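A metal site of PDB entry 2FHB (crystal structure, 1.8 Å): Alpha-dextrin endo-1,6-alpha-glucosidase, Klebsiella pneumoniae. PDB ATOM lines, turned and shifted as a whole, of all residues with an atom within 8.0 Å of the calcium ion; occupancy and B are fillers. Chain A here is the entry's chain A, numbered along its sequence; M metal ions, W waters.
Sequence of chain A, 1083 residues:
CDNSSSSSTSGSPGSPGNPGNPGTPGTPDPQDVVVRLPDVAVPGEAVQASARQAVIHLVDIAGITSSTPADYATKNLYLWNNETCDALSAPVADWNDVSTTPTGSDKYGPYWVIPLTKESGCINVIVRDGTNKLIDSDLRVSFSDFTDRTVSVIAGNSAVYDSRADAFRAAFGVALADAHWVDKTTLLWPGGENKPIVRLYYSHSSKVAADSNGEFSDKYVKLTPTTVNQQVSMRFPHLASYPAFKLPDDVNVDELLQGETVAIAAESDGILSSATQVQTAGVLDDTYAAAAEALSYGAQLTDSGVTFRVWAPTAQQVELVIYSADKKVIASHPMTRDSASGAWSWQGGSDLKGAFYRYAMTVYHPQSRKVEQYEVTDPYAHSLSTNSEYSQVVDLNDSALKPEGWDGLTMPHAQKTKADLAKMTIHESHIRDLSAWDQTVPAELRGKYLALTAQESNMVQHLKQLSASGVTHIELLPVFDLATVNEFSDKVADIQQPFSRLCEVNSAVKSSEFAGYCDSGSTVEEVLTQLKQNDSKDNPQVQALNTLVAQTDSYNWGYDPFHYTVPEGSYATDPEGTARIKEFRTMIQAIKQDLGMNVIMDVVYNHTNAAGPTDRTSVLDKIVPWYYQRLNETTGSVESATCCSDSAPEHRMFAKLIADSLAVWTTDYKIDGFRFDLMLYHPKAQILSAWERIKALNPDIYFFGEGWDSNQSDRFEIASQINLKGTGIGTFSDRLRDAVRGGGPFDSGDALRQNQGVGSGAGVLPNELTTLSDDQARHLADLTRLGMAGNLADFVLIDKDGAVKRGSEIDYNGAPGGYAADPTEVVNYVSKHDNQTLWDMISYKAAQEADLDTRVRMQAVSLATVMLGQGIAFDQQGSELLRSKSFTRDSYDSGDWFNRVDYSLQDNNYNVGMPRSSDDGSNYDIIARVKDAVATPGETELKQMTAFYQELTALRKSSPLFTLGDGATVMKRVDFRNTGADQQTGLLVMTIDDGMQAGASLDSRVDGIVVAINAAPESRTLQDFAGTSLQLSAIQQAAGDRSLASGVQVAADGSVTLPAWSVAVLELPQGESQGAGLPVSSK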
ATOM      1  N   THR A 484      19.528  -8.667 -19.561  1.00  0.00           N
ATOM      2  CA  THR A 484      19.294  -9.012 -20.964  1.00  0.00           C
ATOM      3  C   THR A 484      18.806  -7.966 -21.978  1.00  0.00           C
ATOM      4  O   THR A 484      18.280  -8.319 -23.040  1.00  0.00           O
ATOM      5  CB  THR A 484      18.377 -10.253 -21.018  1.00  0.00           C
ATOM      6  OG1 THR A 484      17.251 -10.060 -20.152  1.00  0.00           O
ATOM      7  CG2 THR A 484      19.139 -11.483 -20.541  1.00  0.00           C
ATOM      8  N   VAL A 485      18.980  -6.690 -21.656  1.00  0.00           N
ATOM      9  CA  VAL A 485      18.643  -5.605 -22.573  1.00  0.00           C
ATOM     10  C   VAL A 485      19.788  -4.611 -22.455  1.00  0.00           C
ATOM     11  O   VAL A 485      20.163  -4.202 -21.345  1.00  0.00           O
ATOM     12  CB  VAL A 485      17.307  -4.911 -22.206  1.00  0.00           C
ATOM     13  CG1 VAL A 485      17.159  -3.622 -23.024  1.00  0.00           C
ATOM     14  CG2 VAL A 485      16.118  -5.829 -22.521  1.00  0.00           C
ATOM     15  N   ASN A 486      20.385  -4.242 -23.586  1.00  0.00           N
ATOM     16  CA  ASN A 486      21.500  -3.302 -23.568  1.00  0.00           C
ATOM     17  C   ASN A 486      20.951  -1.910 -23.308  1.00  0.00           C
ATOM     18  O   ASN A 486      20.084  -1.430 -24.034  1.00  0.00           O
ATOM     19  CB  ASN A 486      22.246  -3.342 -24.907  1.00  0.00           C
ATOM     20  CG  ASN A 486      23.621  -2.689 -24.826  1.00  0.00           C
ATOM     21  OD1 ASN A 486      23.763  -1.584 -24.308  1.00  0.00           O
ATOM     22  ND2 ASN A 486      24.638  -3.381 -25.343  1.00  0.00           N
ATOM     23  N   ASP A 494      14.838  -1.348 -32.485  1.00  0.00           N
ATOM     24  CA  ASP A 494      13.498  -1.884 -32.273  1.00  0.00           C
ATOM     25  C   ASP A 494      12.719  -1.928 -33.579  1.00  0.00           C
ATOM     26  O   ASP A 494      13.073  -1.230 -34.532  1.00  0.00           O
ATOM     27  CB  ASP A 494      12.773  -1.081 -31.193  1.00  0.00           C
ATOM     28  CG  ASP A 494      13.299  -1.395 -29.790  1.00  0.00           C
ATOM     29  OD1 ASP A 494      13.146  -2.551 -29.337  1.00  0.00           O
ATOM     30  OD2 ASP A 494      13.886  -0.497 -29.153  1.00  0.00           O
ATOM     31  N   ASN A 546      12.100 -12.461 -36.608  1.00  0.00           N
ATOM     32  CA  ASN A 546      11.947 -11.974 -35.247  1.00  0.00           C
ATOM     33  C   ASN A 546      12.953 -12.563 -34.268  1.00  0.00           C
ATOM     34  O   ASN A 546      13.374 -11.899 -33.323  1.00  0.00           O
ATOM     35  CB  ASN A 546      10.522 -12.220 -34.733  1.00  0.00           C
ATOM     36  CG  ASN A 546      10.155 -11.304 -33.592  1.00  0.00           C
ATOM     37  OD1 ASN A 546      10.157 -10.082 -33.737  1.00  0.00           O
ATOM     38  ND2 ASN A 546       9.834 -11.882 -32.437  1.00  0.00           N
ATOM     39  N   THR A 547      13.355 -13.820 -34.490  1.00  0.00           N
ATOM     40  CA  THR A 547      14.331 -14.442 -33.611  1.00  0.00           C
ATOM     41  C   THR A 547      15.666 -13.692 -33.636  1.00  0.00           C
ATOM     42  O   THR A 547      16.385 -13.653 -32.650  1.00  0.00           O
ATOM     43  CB  THR A 547      14.568 -15.909 -34.003  1.00  0.00           C
ATOM     44  OG1 THR A 547      13.351 -16.641 -33.801  1.00  0.00           O
ATOM     45  CG2 THR A 547      15.678 -16.529 -33.149  1.00  0.00           C
ATOM     46  N   LEU A 548      15.974 -13.087 -34.781  1.00  0.00           N
ATOM     47  CA  LEU A 548      17.206 -12.317 -34.912  1.00  0.00           C
ATOM     48  C   LEU A 548      16.993 -10.951 -34.264  1.00  0.00           C
ATOM     49  O   LEU A 548      17.864 -10.451 -33.549  1.00  0.00           O
ATOM     50  CB  LEU A 548      17.587 -12.177 -36.393  1.00  0.00           C
ATOM     51  CG  LEU A 548      17.812 -13.523 -37.101  1.00  0.00           C
ATOM     52  CD1 LEU A 548      18.098 -13.307 -38.576  1.00  0.00           C
ATOM     53  CD2 LEU A 548      18.974 -14.253 -36.442  1.00  0.00           C
ATOM     54  N   VAL A 549      15.829 -10.354 -34.506  1.00  0.00           N
ATOM     55  CA  VAL A 549      15.493  -9.058 -33.925  1.00  0.00           C
ATOM     56  C   VAL A 549      15.578  -9.099 -32.388  1.00  0.00           C
ATOM     57  O   VAL A 549      16.035  -8.143 -31.745  1.00  0.00           O
ATOM     58  CB  VAL A 549      14.044  -8.634 -34.302  1.00  0.00           C
ATOM     59  CG1 VAL A 549      13.644  -7.381 -33.521  1.00  0.00           C
ATOM     60  CG2 VAL A 549      13.953  -8.385 -35.803  1.00  0.00           C
ATOM     61  N   ALA A 550      15.152 -10.220 -31.815  1.00  0.00           N
ATOM     62  CA  ALA A 550      15.129 -10.401 -30.368  1.00  0.00           C
ATOM     63  C   ALA A 550      16.485 -10.236 -29.670  1.00  0.00           C
ATOM     64  O   ALA A 550      16.541  -9.904 -28.491  1.00  0.00           O
ATOM     65  CB  ALA A 550      14.535 -11.776 -30.037  1.00  0.00           C
ATOM     66  N   GLN A 551      17.576 -10.465 -30.406  1.00  0.00           N
ATOM     67  CA  GLN A 551      18.923 -10.377 -29.850  1.00  0.00           C
ATOM     68  C   GLN A 551      19.400  -8.969 -29.536  1.00  0.00           C
ATOM     69  O   GLN A 551      20.240  -8.773 -28.649  1.00  0.00           O
ATOM     70  CB  GLN A 551      19.924 -11.011 -30.825  1.00  0.00           C
ATOM     71  CG  GLN A 551      19.628 -12.447 -31.217  1.00  0.00           C
ATOM     72  CD  GLN A 551      20.534 -12.944 -32.325  1.00  0.00           C
ATOM     73  OE1 GLN A 551      20.524 -14.124 -32.669  1.00  0.00           O
ATOM     74  NE2 GLN A 551      21.329 -12.040 -32.887  1.00  0.00           N
ATOM     75  N   THR A 552      18.860  -7.985 -30.259  1.00  0.00           N
ATOM     76  CA  THR A 552      19.293  -6.605 -30.073  1.00  0.00           C
ATOM     77  C   THR A 552      18.185  -5.572 -29.874  1.00  0.00           C
ATOM     78  O   THR A 552      18.414  -4.379 -30.067  1.00  0.00           O
ATOM     79  CB  THR A 552      20.173  -6.155 -31.283  1.00  0.00           C
ATOM     80  OG1 THR A 552      19.511  -6.468 -32.510  1.00  0.00           O
ATOM     81  CG2 THR A 552      21.523  -6.860 -31.261  1.00  0.00           C
ATOM     82  N   ASP A 553      16.995  -6.019 -29.475  1.00  0.00           N
ATOM     83  CA  ASP A 553      15.889  -5.099 -29.249  1.00  0.00           C
ATOM     84  C   ASP A 553      15.821  -4.687 -27.773  1.00  0.00           C
ATOM     85  O   ASP A 553      16.693  -5.043 -26.993  1.00  0.00           O
ATOM     86  CB  ASP A 553      14.536  -5.701 -29.709  1.00  0.00           C
ATOM     87  CG  ASP A 553      14.136  -6.975 -28.951  1.00  0.00           C
ATOM     88  OD1 ASP A 553      14.673  -7.258 -27.857  1.00  0.00           O
ATOM     89  OD2 ASP A 553      13.243  -7.687 -29.461  1.00  0.00           O
ATOM     90  N   SER A 554      14.797  -3.923 -27.404  1.00  0.00           N
ATOM     91  CA  SER A 554      14.636  -3.464 -26.023  1.00  0.00           C
ATOM     92  C   SER A 554      13.728  -4.381 -25.217  1.00  0.00           C
ATOM     93  O   SER A 554      13.340  -4.060 -24.093  1.00  0.00           O
ATOM     94  CB  SER A 554      14.020  -2.061 -26.000  1.00  0.00           C
ATOM     95  OG  SER A 554      14.828  -1.121 -26.692  1.00  0.00           O
ATOM     96  N   TYR A 555      13.402  -5.544 -25.770  1.00  0.00           N
ATOM     97  CA  TYR A 555      12.462  -6.448 -25.113  1.00  0.00           C
ATOM     98  C   TYR A 555      12.950  -7.705 -24.406  1.00  0.00           C
ATOM     99  O   TYR A 555      13.753  -8.461 -24.927  1.00  0.00           O
ATOM    100  CB  TYR A 555      11.369  -6.834 -26.127  1.00  0.00           C
ATOM    101  CG  TYR A 555      10.149  -7.454 -25.481  1.00  0.00           C
ATOM    102  CD1 TYR A 555      10.174  -8.757 -24.969  1.00  0.00           C
ATOM    103  CD2 TYR A 555       8.989  -6.695 -25.298  1.00  0.00           C
ATOM    104  CE1 TYR A 555       9.080  -9.270 -24.275  1.00  0.00           C
ATOM    105  CE2 TYR A 555       7.895  -7.207 -24.613  1.00  0.00           C
ATOM    106  CZ  TYR A 555       7.943  -8.488 -24.092  1.00  0.00           C
ATOM    107  OH  TYR A 555       6.894  -8.957 -23.358  1.00  0.00           O
ATOM    108  N   ASN A 556      12.403  -7.906 -23.201  1.00  0.00           N
ATOM    109  CA  ASN A 556      12.649  -9.100 -22.384  1.00  0.00           C
ATOM    110  C   ASN A 556      11.806  -9.006 -21.110  1.00  0.00           C
ATOM    111  O   ASN A 556      11.646  -7.923 -20.552  1.00  0.00           O
ATOM    112  CB  ASN A 556      14.126  -9.273 -22.021  1.00  0.00           C
ATOM    113  CG  ASN A 556      14.467 -10.714 -21.624  1.00  0.00           C
ATOM    114  OD1 ASN A 556      14.043 -11.205 -20.573  1.00  0.00           O
ATOM    115  ND2 ASN A 556      15.236 -11.395 -22.462  1.00  0.00           N
ATOM    116  N   TRP A 557      11.255 -10.129 -20.663  1.00  0.00           N
ATOM    117  CA  TRP A 557      10.470 -10.127 -19.434  1.00  0.00           C
ATOM    118  C   TRP A 557      11.373  -9.629 -18.310  1.00  0.00           C
ATOM    119  O   TRP A 557      10.924  -8.935 -17.403  1.00  0.00           O
ATOM    120  CB  TRP A 557       9.986 -11.537 -19.068  1.00  0.00           C
ATOM    121  CG  TRP A 557       8.804 -12.025 -19.841  1.00  0.00           C
ATOM    122  CD1 TRP A 557       7.947 -11.302 -20.621  1.00  0.00           C
ATOM    123  CD2 TRP A 557       8.327 -13.379 -19.874  1.00  0.00           C
ATOM    124  NE1 TRP A 557       6.982 -12.117 -21.151  1.00  0.00           N
ATOM    125  CE2 TRP A 557       7.198 -13.400 -20.706  1.00  0.00           C
ATOM    126  CE3 TRP A 557       8.770 -14.574 -19.294  1.00  0.00           C
ATOM    127  CZ2 TRP A 557       6.479 -14.574 -20.965  1.00  0.00           C
ATOM    128  CZ3 TRP A 557       8.060 -15.744 -19.553  1.00  0.00           C
ATOM    129  CH2 TRP A 557       6.935 -15.729 -20.384  1.00  0.00           C
ATOM    130  N   TYR A 892       9.013 -14.817 -23.414  1.00  0.00           N
ATOM    131  CA  TYR A 892       9.974 -13.944 -22.722  1.00  0.00           C
ATOM    132  C   TYR A 892      10.912 -13.110 -23.581  1.00  0.00           C
ATOM    133  O   TYR A 892      11.323 -12.010 -23.163  1.00  0.00           O
ATOM    134  CB  TYR A 892      10.817 -14.763 -21.724  1.00  0.00           C
ATOM    135  CG  TYR A 892      11.929 -15.558 -22.377  1.00  0.00           C
ATOM    136  CD1 TYR A 892      11.640 -16.692 -23.141  1.00  0.00           C
ATOM    137  CD2 TYR A 892      13.255 -15.158 -22.242  1.00  0.00           C
ATOM    138  CE1 TYR A 892      12.667 -17.408 -23.769  1.00  0.00           C
ATOM    139  CE2 TYR A 892      14.291 -15.869 -22.870  1.00  0.00           C
ATOM    140  CZ  TYR A 892      13.984 -16.990 -23.623  1.00  0.00           C
ATOM    141  OH  TYR A 892      14.998 -17.680 -24.240  1.00  0.00           O
ATOM    142  N   ASP A 893      11.255 -13.609 -24.759  1.00  0.00           N
ATOM    143  CA  ASP A 893      12.166 -12.900 -25.661  1.00  0.00           C
ATOM    144  C   ASP A 893      11.548 -12.801 -27.058  1.00  0.00           C
ATOM    145  O   ASP A 893      12.273 -12.654 -28.041  1.00  0.00           O
ATOM    146  CB  ASP A 893      13.504 -13.652 -25.721  1.00  0.00           C
ATOM    147  CG  ASP A 893      14.661 -12.792 -26.207  1.00  0.00           C
ATOM    148  OD1 ASP A 893      15.715 -13.373 -26.531  1.00  0.00           O
ATOM    149  OD2 ASP A 893      14.531 -11.552 -26.266  1.00  0.00           O
ATOM    150  N   SER A 894      10.216 -12.858 -27.143  1.00  0.00           N
ATOM    151  CA  SER A 894       9.530 -12.799 -28.438  1.00  0.00           C
ATOM    152  C   SER A 894       9.192 -11.387 -28.906  1.00  0.00           C
ATOM    153  O   SER A 894       8.415 -11.200 -29.844  1.00  0.00           O
ATOM    154  CB  SER A 894       8.281 -13.673 -28.430  1.00  0.00           C
ATOM    155  OG  SER A 894       8.636 -15.045 -28.363  1.00  0.00           O
ATOM    156  N   GLY A 895       9.771 -10.405 -28.227  1.00  0.00           N
ATOM    157  CA  GLY A 895       9.612  -9.009 -28.581  1.00  0.00           C
ATOM    158  C   GLY A 895       8.257  -8.338 -28.633  1.00  0.00           C
ATOM    159  O   GLY A 895       7.235  -8.870 -28.172  1.00  0.00           O
ATOM    160  N   ASP A 896       8.257  -7.132 -29.189  1.00  0.00           N
ATOM    161  CA  ASP A 896       7.051  -6.337 -29.313  1.00  0.00           C
ATOM    162  C   ASP A 896       6.032  -7.016 -30.218  1.00  0.00           C
ATOM    163  O   ASP A 896       4.830  -6.876 -30.001  1.00  0.00           O
ATOM    164  CB  ASP A 896       7.362  -4.948 -29.904  1.00  0.00           C
ATOM    165  CG  ASP A 896       8.113  -4.048 -28.943  1.00  0.00           C
ATOM    166  OD1 ASP A 896       8.117  -4.317 -27.730  1.00  0.00           O
ATOM    167  OD2 ASP A 896       8.687  -3.036 -29.414  1.00  0.00           O
HETATM  168 CA    CA M   1      15.190  -9.315 -26.544  1.00  0.00          CA
HETATM  169  O   HOH W   1      12.974  -9.755 -27.830  1.00  0.00           O
HETATM  170  O   HOH W   2      16.828  -7.573 -25.971  1.00  0.00           O
HETATM  171  O   HOH W   3      16.676 -10.038 -24.686  1.00  0.00           O
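Four residues have an atom within 4 Å of the calcium ion: Ala 550, Asp 553, Tyr 555 and Asp 893.
The backbone carbonyl oxygen (O) of Tyr 555 is bound to the calcium ion (2.3 Å).
The calcium ion is bound by the side-chain carboxylate (OD2) of Asp 893, 2.3 Å away.
O of Ala 550 binds the calcium ion (2.4 Å).
Water W2 binds the calcium ion (2.5 Å).
Water W3 binds the calcium ion.
The calcium ion is bound by the side-chain carboxylate (OD1) of Asp 553, 2.5 Å away.
Water W1 is bound to the calcium ion, 2.6 Å away.
Water W2 bridges the backbone carbonyl oxygen (O) of Asp 553 (2.7 Å) and the backbone carbonyl oxygen (O) of Thr 484 (3.4 Å).
Water W3 bridges the backbone carbonyl oxygen (O) of Thr 484 (2.9 Å) and the side-chain amide nitrogen (ND2) of Asn 556 (3.0 Å).
Water W1 lies within hydrogen-bond range of the side-chain carboxylate of Asp 553, the backbone carbonyl oxygen of Asp 893 and the backbone NH of Gly 895.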
